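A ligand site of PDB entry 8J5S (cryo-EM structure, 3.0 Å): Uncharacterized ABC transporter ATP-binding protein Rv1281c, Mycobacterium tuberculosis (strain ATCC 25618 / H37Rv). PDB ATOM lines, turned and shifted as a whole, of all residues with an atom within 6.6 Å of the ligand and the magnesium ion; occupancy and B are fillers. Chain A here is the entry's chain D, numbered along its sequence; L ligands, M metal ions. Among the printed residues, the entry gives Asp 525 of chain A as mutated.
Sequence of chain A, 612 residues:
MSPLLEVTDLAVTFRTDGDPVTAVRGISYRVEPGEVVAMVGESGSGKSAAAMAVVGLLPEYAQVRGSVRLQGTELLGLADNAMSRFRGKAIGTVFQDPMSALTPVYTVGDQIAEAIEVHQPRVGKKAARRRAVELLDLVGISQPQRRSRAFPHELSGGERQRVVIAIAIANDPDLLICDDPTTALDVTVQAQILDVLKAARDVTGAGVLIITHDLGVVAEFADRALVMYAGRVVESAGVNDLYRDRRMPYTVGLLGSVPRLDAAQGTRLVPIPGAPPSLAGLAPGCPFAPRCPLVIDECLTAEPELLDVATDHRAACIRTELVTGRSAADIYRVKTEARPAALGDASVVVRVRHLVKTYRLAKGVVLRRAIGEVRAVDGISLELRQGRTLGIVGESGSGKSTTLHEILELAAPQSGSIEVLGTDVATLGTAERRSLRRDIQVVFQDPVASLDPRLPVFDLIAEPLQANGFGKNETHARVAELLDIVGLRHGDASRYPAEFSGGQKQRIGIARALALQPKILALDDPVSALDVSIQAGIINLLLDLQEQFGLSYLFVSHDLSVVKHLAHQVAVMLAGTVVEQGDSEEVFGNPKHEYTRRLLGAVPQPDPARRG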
ATOM      1  N   ASP A 186      -2.842   8.466  -9.218  1.00  0.00           N
ATOM      2  CA  ASP A 186      -1.730   8.203 -10.096  1.00  0.00           C
ATOM      3  C   ASP A 186      -0.469   8.045  -9.265  1.00  0.00           C
ATOM      4  O   ASP A 186      -0.515   7.996  -8.035  1.00  0.00           O
ATOM      5  CB  ASP A 186      -1.603   9.305 -11.138  1.00  0.00           C
ATOM      6  CG  ASP A 186      -1.075  10.590 -10.557  1.00  0.00           C
ATOM      7  OD1 ASP A 186       0.163  10.763 -10.510  1.00  0.00           O
ATOM      8  OD2 ASP A 186      -1.896  11.446 -10.176  1.00  0.00           O
ATOM      9  N   TYR A 359     -11.315  23.041 -24.972  1.00  0.00           N
ATOM     10  CA  TYR A 359     -12.731  23.106 -24.607  1.00  0.00           C
ATOM     11  C   TYR A 359     -13.068  24.525 -24.159  1.00  0.00           C
ATOM     12  O   TYR A 359     -12.307  25.149 -23.418  1.00  0.00           O
ATOM     13  CB  TYR A 359     -13.084  22.122 -23.492  1.00  0.00           C
ATOM     14  CG  TYR A 359     -12.559  20.722 -23.656  1.00  0.00           C
ATOM     15  CD1 TYR A 359     -13.367  19.706 -24.133  1.00  0.00           C
ATOM     16  CD2 TYR A 359     -11.258  20.404 -23.291  1.00  0.00           C
ATOM     17  CE1 TYR A 359     -12.885  18.422 -24.264  1.00  0.00           C
ATOM     18  CE2 TYR A 359     -10.783  19.131 -23.419  1.00  0.00           C
ATOM     19  CZ  TYR A 359     -11.595  18.140 -23.900  1.00  0.00           C
ATOM     20  OH  TYR A 359     -11.100  16.860 -24.022  1.00  0.00           O
ATOM     21  N   ARG A 360     -14.217  25.018 -24.602  1.00  0.00           N
ATOM     22  CA  ARG A 360     -14.697  26.326 -24.166  1.00  0.00           C
ATOM     23  C   ARG A 360     -15.244  26.181 -22.753  1.00  0.00           C
ATOM     24  O   ARG A 360     -16.287  25.568 -22.534  1.00  0.00           O
ATOM     25  CB  ARG A 360     -15.762  26.845 -25.125  1.00  0.00           C
ATOM     26  CG  ARG A 360     -15.315  26.934 -26.576  1.00  0.00           C
ATOM     27  CD  ARG A 360     -13.875  27.407 -26.692  1.00  0.00           C
ATOM     28  NE  ARG A 360     -13.354  27.286 -28.056  1.00  0.00           N
ATOM     29  CZ  ARG A 360     -12.920  26.149 -28.593  1.00  0.00           C
ATOM     30  NH1 ARG A 360     -12.467  26.138 -29.838  1.00  0.00           N
ATOM     31  NH2 ARG A 360     -12.936  25.034 -27.892  1.00  0.00           N
ATOM     32  N   LEU A 361     -14.521  26.760 -21.788  1.00  0.00           N
ATOM     33  CA  LEU A 361     -14.819  26.519 -20.373  1.00  0.00           C
ATOM     34  C   LEU A 361     -16.182  27.067 -19.994  1.00  0.00           C
ATOM     35  O   LEU A 361     -16.653  28.074 -20.536  1.00  0.00           O
ATOM     36  CB  LEU A 361     -13.739  27.142 -19.497  1.00  0.00           C
ATOM     37  CG  LEU A 361     -12.667  26.172 -18.991  1.00  0.00           C
ATOM     38  CD1 LEU A 361     -11.698  26.888 -18.066  1.00  0.00           C
ATOM     39  CD2 LEU A 361     -13.303  24.990 -18.299  1.00  0.00           C
ATOM     40  N   ALA A 362     -16.823  26.389 -19.045  1.00  0.00           N
ATOM     41  CA  ALA A 362     -18.141  26.785 -18.551  1.00  0.00           C
ATOM     42  C   ALA A 362     -18.146  26.696 -17.036  1.00  0.00           C
ATOM     43  O   ALA A 362     -17.842  25.644 -16.466  1.00  0.00           O
ATOM     44  CB  ALA A 362     -19.238  25.897 -19.151  1.00  0.00           C
ATOM     45  N   VAL A 374      -9.676  25.686 -20.995  1.00  0.00           N
ATOM     46  CA  VAL A 374      -8.698  24.624 -20.836  1.00  0.00           C
ATOM     47  C   VAL A 374      -8.086  24.299 -22.186  1.00  0.00           C
ATOM     48  O   VAL A 374      -8.806  24.153 -23.191  1.00  0.00           O
ATOM     49  CB  VAL A 374      -9.329  23.382 -20.179  1.00  0.00           C
ATOM     50  CG1 VAL A 374      -9.979  23.745 -18.855  1.00  0.00           C
ATOM     51  CG2 VAL A 374     -10.345  22.742 -21.079  1.00  0.00           C
ATOM     52  N   ARG A 375      -6.767  24.245 -22.233  1.00  0.00           N
ATOM     53  CA  ARG A 375      -6.044  23.814 -23.428  1.00  0.00           C
ATOM     54  C   ARG A 375      -5.585  22.395 -23.149  1.00  0.00           C
ATOM     55  O   ARG A 375      -4.480  22.155 -22.664  1.00  0.00           O
ATOM     56  CB  ARG A 375      -4.876  24.749 -23.710  1.00  0.00           C
ATOM     57  CG  ARG A 375      -4.433  24.753 -25.158  1.00  0.00           C
ATOM     58  CD  ARG A 375      -3.832  26.090 -25.551  1.00  0.00           C
ATOM     59  NE  ARG A 375      -3.850  26.291 -26.986  1.00  0.00           N
ATOM     60  CZ  ARG A 375      -2.766  26.475 -27.730  1.00  0.00           C
ATOM     61  NH1 ARG A 375      -1.566  26.488 -27.163  1.00  0.00           N
ATOM     62  NH2 ARG A 375      -2.870  26.653 -29.042  1.00  0.00           N
ATOM     63  N   ALA A 376      -6.467  21.428 -23.449  1.00  0.00           N
ATOM     64  CA  ALA A 376      -6.214  20.044 -23.089  1.00  0.00           C
ATOM     65  C   ALA A 376      -4.993  19.494 -23.809  1.00  0.00           C
ATOM     66  O   ALA A 376      -4.170  18.797 -23.213  1.00  0.00           O
ATOM     67  CB  ALA A 376      -7.436  19.193 -23.391  1.00  0.00           C
ATOM     68  N   VAL A 377      -4.859  19.800 -25.089  1.00  0.00           N
ATOM     69  CA  VAL A 377      -3.711  19.369 -25.865  1.00  0.00           C
ATOM     70  C   VAL A 377      -3.043  20.607 -26.446  1.00  0.00           C
ATOM     71  O   VAL A 377      -3.689  21.646 -26.622  1.00  0.00           O
ATOM     72  CB  VAL A 377      -4.118  18.375 -26.961  1.00  0.00           C
ATOM     73  CG1 VAL A 377      -2.914  17.842 -27.685  1.00  0.00           C
ATOM     74  CG2 VAL A 377      -4.892  17.233 -26.363  1.00  0.00           C
ATOM     75  N   GLY A 394       1.293   9.767 -17.707  1.00  0.00           N
ATOM     76  CA  GLY A 394       1.299  11.100 -17.187  1.00  0.00           C
ATOM     77  C   GLY A 394       0.670  11.139 -15.814  1.00  0.00           C
ATOM     78  O   GLY A 394       0.571  10.119 -15.131  1.00  0.00           O
ATOM     79  N   GLU A 395       0.256  12.332 -15.403  1.00  0.00           N
ATOM     80  CA  GLU A 395      -0.529  12.516 -14.201  1.00  0.00           C
ATOM     81  C   GLU A 395      -1.919  12.974 -14.582  1.00  0.00           C
ATOM     82  O   GLU A 395      -2.176  13.336 -15.726  1.00  0.00           O
ATOM     83  CB  GLU A 395       0.156  13.532 -13.279  1.00  0.00           C
ATOM     84  CG  GLU A 395       1.648  13.398 -13.257  1.00  0.00           C
ATOM     85  CD  GLU A 395       2.349  14.585 -12.631  1.00  0.00           C
ATOM     86  OE1 GLU A 395       1.682  15.606 -12.404  1.00  0.00           O
ATOM     87  OE2 GLU A 395       3.564  14.484 -12.371  1.00  0.00           O
ATOM     88  N   SER A 396      -2.836  12.931 -13.616  1.00  0.00           N
ATOM     89  CA  SER A 396      -4.213  13.295 -13.907  1.00  0.00           C
ATOM     90  C   SER A 396      -4.278  14.719 -14.433  1.00  0.00           C
ATOM     91  O   SER A 396      -3.681  15.642 -13.870  1.00  0.00           O
ATOM     92  CB  SER A 396      -5.070  13.165 -12.658  1.00  0.00           C
ATOM     93  OG  SER A 396      -6.314  13.817 -12.835  1.00  0.00           O
ATOM     94  N   GLY A 397      -5.009  14.891 -15.533  1.00  0.00           N
ATOM     95  CA  GLY A 397      -5.126  16.173 -16.196  1.00  0.00           C
ATOM     96  C   GLY A 397      -4.187  16.369 -17.360  1.00  0.00           C
ATOM     97  O   GLY A 397      -4.244  17.416 -18.012  1.00  0.00           O
ATOM     98  N   SER A 398      -3.343  15.386 -17.659  1.00  0.00           N
ATOM     99  CA  SER A 398      -2.327  15.555 -18.686  1.00  0.00           C
ATOM    100  C   SER A 398      -2.954  15.780 -20.059  1.00  0.00           C
ATOM    101  O   SER A 398      -2.519  16.654 -20.808  1.00  0.00           O
ATOM    102  CB  SER A 398      -1.406  14.340 -18.717  1.00  0.00           C
ATOM    103  OG  SER A 398      -0.648  14.345 -19.904  1.00  0.00           O
ATOM    104  N   GLY A 399      -3.945  14.956 -20.414  1.00  0.00           N
ATOM    105  CA  GLY A 399      -4.633  15.106 -21.722  1.00  0.00           C
ATOM    106  C   GLY A 399      -4.585  13.827 -22.549  1.00  0.00           C
ATOM    107  O   GLY A 399      -5.020  13.871 -23.734  1.00  0.00           O
ATOM    108  N   LYS A 400      -4.109  12.723 -21.956  1.00  0.00           N
ATOM    109  CA  LYS A 400      -3.967  11.441 -22.695  1.00  0.00           C
ATOM    110  C   LYS A 400      -5.330  11.004 -23.278  1.00  0.00           C
ATOM    111  O   LYS A 400      -5.368  10.682 -24.482  1.00  0.00           O
ATOM    112  CB  LYS A 400      -3.413  10.372 -21.754  1.00  0.00           C
ATOM    113  CG  LYS A 400      -2.132  10.779 -21.020  1.00  0.00           C
ATOM    114  CD  LYS A 400      -1.770   9.848 -19.883  1.00  0.00           C
ATOM    115  CE  LYS A 400      -2.778   9.874 -18.753  1.00  0.00           C
ATOM    116  NZ  LYS A 400      -2.924  11.227 -18.173  1.00  0.00           N
ATOM    117  N   SER A 401      -6.377  10.986 -22.451  1.00  0.00           N
ATOM    118  CA  SER A 401      -7.713  10.522 -22.920  1.00  0.00           C
ATOM    119  C   SER A 401      -8.224  11.435 -24.036  1.00  0.00           C
ATOM    120  O   SER A 401      -8.807  10.907 -25.013  1.00  0.00           O
ATOM    121  CB  SER A 401      -8.693  10.449 -21.774  1.00  0.00           C
ATOM    122  OG  SER A 401      -9.960   9.992 -22.231  1.00  0.00           O
ATOM    123  N   THR A 402      -8.011  12.750 -23.896  1.00  0.00           N
ATOM    124  CA  THR A 402      -8.442  13.712 -24.952  1.00  0.00           C
ATOM    125  C   THR A 402      -7.769  13.319 -26.276  1.00  0.00           C
ATOM    126  O   THR A 402      -8.492  13.194 -27.276  1.00  0.00           O
ATOM    127  CB  THR A 402      -8.091  15.152 -24.557  1.00  0.00           C
ATOM    128  OG1 THR A 402      -8.814  15.476 -23.365  1.00  0.00           O
ATOM    129  CG2 THR A 402      -8.399  16.152 -25.646  1.00  0.00           C
ATOM    130  N   THR A 403      -6.452  13.093 -26.246  1.00  0.00           N
ATOM    131  CA  THR A 403      -5.710  12.715 -27.473  1.00  0.00           C
ATOM    132  C   THR A 403      -6.265  11.391 -28.028  1.00  0.00           C
ATOM    133  O   THR A 403      -6.471  11.311 -29.256  1.00  0.00           O
ATOM    134  CB  THR A 403      -4.209  12.586 -27.182  1.00  0.00           C
ATOM    135  OG1 THR A 403      -3.787  13.791 -26.539  1.00  0.00           O
ATOM    136  CG2 THR A 403      -3.390  12.334 -28.425  1.00  0.00           C
ATOM    137  N   GLN A 445     -12.077   4.125 -20.487  1.00  0.00           N
ATOM    138  CA  GLN A 445     -11.391   4.133 -19.165  1.00  0.00           C
ATOM    139  C   GLN A 445     -12.357   3.679 -18.064  1.00  0.00           C
ATOM    140  O   GLN A 445     -11.978   2.791 -17.283  1.00  0.00           O
ATOM    141  CB  GLN A 445     -10.832   5.519 -18.867  1.00  0.00           C
ATOM    142  CG  GLN A 445      -9.855   5.553 -17.710  1.00  0.00           C
ATOM    143  CD  GLN A 445      -9.102   6.868 -17.635  1.00  0.00           C
ATOM    144  OE1 GLN A 445      -9.299   7.754 -18.456  1.00  0.00           O
ATOM    145  NE2 GLN A 445      -8.228   6.976 -16.653  1.00  0.00           N
ATOM    146  N   ASP A 524      -7.725   2.609 -22.666  1.00  0.00           N
ATOM    147  CA  ASP A 524      -7.672   3.677 -21.674  1.00  0.00           C
ATOM    148  C   ASP A 524      -7.709   3.042 -20.284  1.00  0.00           C
ATOM    149  O   ASP A 524      -8.770   2.926 -19.673  1.00  0.00           O
ATOM    150  CB  ASP A 524      -8.820   4.664 -21.874  1.00  0.00           C
ATOM    151  CG  ASP A 524      -8.448   6.093 -21.516  1.00  0.00           C
ATOM    152  OD1 ASP A 524      -7.396   6.317 -20.889  1.00  0.00           O
ATOM    153  OD2 ASP A 524      -9.234   7.002 -21.854  1.00  0.00           O
ATOM    154  N   ASP A 525      -6.538   2.649 -19.780  1.00  0.00           N
ATOM    155  CA  ASP A 525      -6.381   1.987 -18.489  1.00  0.00           C
ATOM    156  C   ASP A 525      -7.384   0.848 -18.341  1.00  0.00           C
ATOM    157  O   ASP A 525      -8.292   0.931 -17.504  1.00  0.00           O
ATOM    158  CB  ASP A 525      -6.559   2.991 -17.349  1.00  0.00           C
ATOM    159  CG  ASP A 525      -5.697   2.651 -16.153  1.00  0.00           C
ATOM    160  OD1 ASP A 525      -5.721   3.424 -15.160  1.00  0.00           O
ATOM    161  OD2 ASP A 525      -4.987   1.627 -16.190  1.00  0.00           O
ATOM    162  N   VAL A 556      -2.518   3.458 -22.546  1.00  0.00           N
ATOM    163  CA  VAL A 556      -2.307   4.429 -21.485  1.00  0.00           C
ATOM    164  C   VAL A 556      -2.674   3.778 -20.160  1.00  0.00           C
ATOM    165  O   VAL A 556      -3.599   2.971 -20.107  1.00  0.00           O
ATOM    166  CB  VAL A 556      -3.124   5.714 -21.704  1.00  0.00           C
ATOM    167  CG1 VAL A 556      -2.836   6.299 -23.052  1.00  0.00           C
ATOM    168  CG2 VAL A 556      -4.563   5.417 -21.623  1.00  0.00           C
ATOM    169  N   MET A 573       4.068  12.464 -21.071  1.00  0.00           N
ATOM    170  CA  MET A 573       3.329  13.624 -21.538  1.00  0.00           C
ATOM    171  C   MET A 573       2.848  14.432 -20.340  1.00  0.00           C
ATOM    172  O   MET A 573       2.216  13.887 -19.437  1.00  0.00           O
ATOM    173  CB  MET A 573       2.166  13.178 -22.403  1.00  0.00           C
ATOM    174  CG  MET A 573       1.000  14.094 -22.399  1.00  0.00           C
ATOM    175  SD  MET A 573      -0.158  13.765 -23.726  1.00  0.00           S
ATOM    176  CE  MET A 573      -1.376  14.985 -23.316  1.00  0.00           C
HETATM  177  P1  LIG L   1      -6.523  10.397 -16.920  1.00  0.00           P
HETATM  178  O1  LIG L   1      -7.674   9.908 -16.066  1.00  0.00           O
HETATM  179  O2  LIG L   1      -6.216   9.354 -17.955  1.00  0.00           O
HETATM  180  O3  LIG L   1      -5.311  10.569 -16.040  1.00  0.00           O
HETATM  181  P2  LIG L   1      -5.918  12.684 -18.608  1.00  0.00           P
HETATM  182  O4  LIG L   1      -4.692  13.152 -17.872  1.00  0.00           O
HETATM  183  O5  LIG L   1      -5.738  12.011 -19.945  1.00  0.00           O
HETATM  184  N1  LIG L   1      -6.908  11.821 -17.634  1.00  0.00           N
HETATM  185  P3  LIG L   1      -8.088  14.244 -19.794  1.00  0.00           P
HETATM  186  O6  LIG L   1      -7.790  13.963 -21.219  1.00  0.00           O
HETATM  187  O7  LIG L   1      -9.211  13.499 -19.135  1.00  0.00           O
HETATM  188  O8  LIG L   1      -6.758  14.004 -18.929  1.00  0.00           O
HETATM  189  O9  LIG L   1      -8.305  15.822 -19.588  1.00  0.00           O
HETATM  190  C1  LIG L   1      -7.195  16.714 -19.881  1.00  0.00           C
HETATM  191  C2  LIG L   1      -7.664  18.138 -19.783  1.00  0.00           C
HETATM  192  O10 LIG L   1      -8.898  18.295 -20.536  1.00  0.00           O
HETATM  193  C3  LIG L   1      -7.977  18.661 -18.365  1.00  0.00           C
HETATM  194  O11 LIG L   1      -7.553  20.000 -18.221  1.00  0.00           O
HETATM  195  C4  LIG L   1      -9.511  18.560 -18.307  1.00  0.00           C
HETATM  196  O12 LIG L   1     -10.092  19.433 -17.359  1.00  0.00           O
HETATM  197  C5  LIG L   1      -9.855  18.957 -19.740  1.00  0.00           C
HETATM  198  N2  LIG L   1     -11.165  18.509 -20.168  1.00  0.00           N
HETATM  199  C6  LIG L   1     -11.515  17.260 -20.625  1.00  0.00           C
HETATM  200  N3  LIG L   1     -12.796  17.178 -20.935  1.00  0.00           N
HETATM  201  C7  LIG L   1     -13.303  18.447 -20.658  1.00  0.00           C
HETATM  202  C8  LIG L   1     -14.587  18.998 -20.788  1.00  0.00           C
HETATM  203  N4  LIG L   1     -15.645  18.327 -21.222  1.00  0.00           N
HETATM  204  N5  LIG L   1     -14.746  20.296 -20.426  1.00  0.00           N
HETATM  205  C9  LIG L   1     -13.674  20.971 -19.983  1.00  0.00           C
HETATM  206  N6  LIG L   1     -12.418  20.553 -19.829  1.00  0.00           N
HETATM  207  C10 LIG L   1     -12.299  19.270 -20.193  1.00  0.00           C
HETATM  208 MG    MG M   1      -8.865  10.057 -18.796  1.00  0.00          MG
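An oxygen (O6) of the ligand sits at hydrogen-bond distance from the side-chain hydroxyl (OG1) of Thr 402 (2.8 Å).
The backbone NH of Lys 400 lies within hydrogen-bond range of an oxygen (O5) of the ligand (2.7 Å).
N of Ser 398 sits at hydrogen-bond distance from O4 of the ligand.
NE2 of Gln 445 lies within hydrogen-bond range of O1 of the ligand, at 3.0 Å.
The backbone NH (N) of Thr 402 is in hydrogen-bond range of an oxygen (O6) of the ligand (2.9 Å).
N of Ser 401 sits at hydrogen-bond distance from O5 of the ligand (2.8 Å).
An oxygen (O4) of the ligand is in salt-bridge range of the side-chain amino group (NZ) of Lys 400 (2.6 Å).
The backbone NH (N) of Gly 399 is in hydrogen-bond range of an oxygen (O4) of the ligand, 3.2 Å away.
The backbone NH (N) of Gly 397 lies within hydrogen-bond range of an oxygen (O4) of the ligand (2.9 Å).
The side-chain carboxylate of Asp 524 lies within hydrogen-bond range of the side-chain hydroxyl of Ser 401, 3.1 Å away.
The side-chain hydroxyl of Ser 398 sits at hydrogen-bond distance from the backbone carbonyl oxygen of Met 573, at 2.9 Å.
O of Gly 399 lies within hydrogen-bond range of OG1 of Thr 403, 3.1 Å away.
The side-chain carboxylate of Asp 524 sits close to the side-chain amide oxygen of Gln 445 (3.4 Å).
The backbone NH of Tyr 359 lies within hydrogen-bond range of the backbone carbonyl oxygen of Val 374, at 3.3 Å.
The side-chain amino group of Lys 400 is in hydrogen-bond range of the backbone carbonyl oxygen of Glu 395 (3.3 Å).
The side-chain hydroxyl (OH) of Tyr 359 lies within hydrogen-bond range of the side-chain hydroxyl (OG1) of Thr 402 (2.8 Å).
O of Glu 395 sits close to O4 of the ligand (3.3 Å).
Residues that only touch the ligand: Val 374 (3.3 Å), Ala 376 (3.3 Å), Tyr 359 (3.3 Å) and Ser 396 (3.6 Å).
Hydrophobic or aromatic side chains within 4 Å of the ligand: Tyr 359, Val 374 and Ala 376.
Of the 24 residues printed, 12 come within 4 Å of the ligand.
The nearest printed residue that does not touch the ligand is Leu 361 (4.4 Å).
Ser 401 touches the magnesium ion (CB to MG, 3.0 Å).
Within 4 Å of the magnesium ion: Ser 401 and Gln 445.
The magnesium ion is bound by OE1 of Gln 445 (2.4 Å).
The magnesium ion has one donor atom within binding distance.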
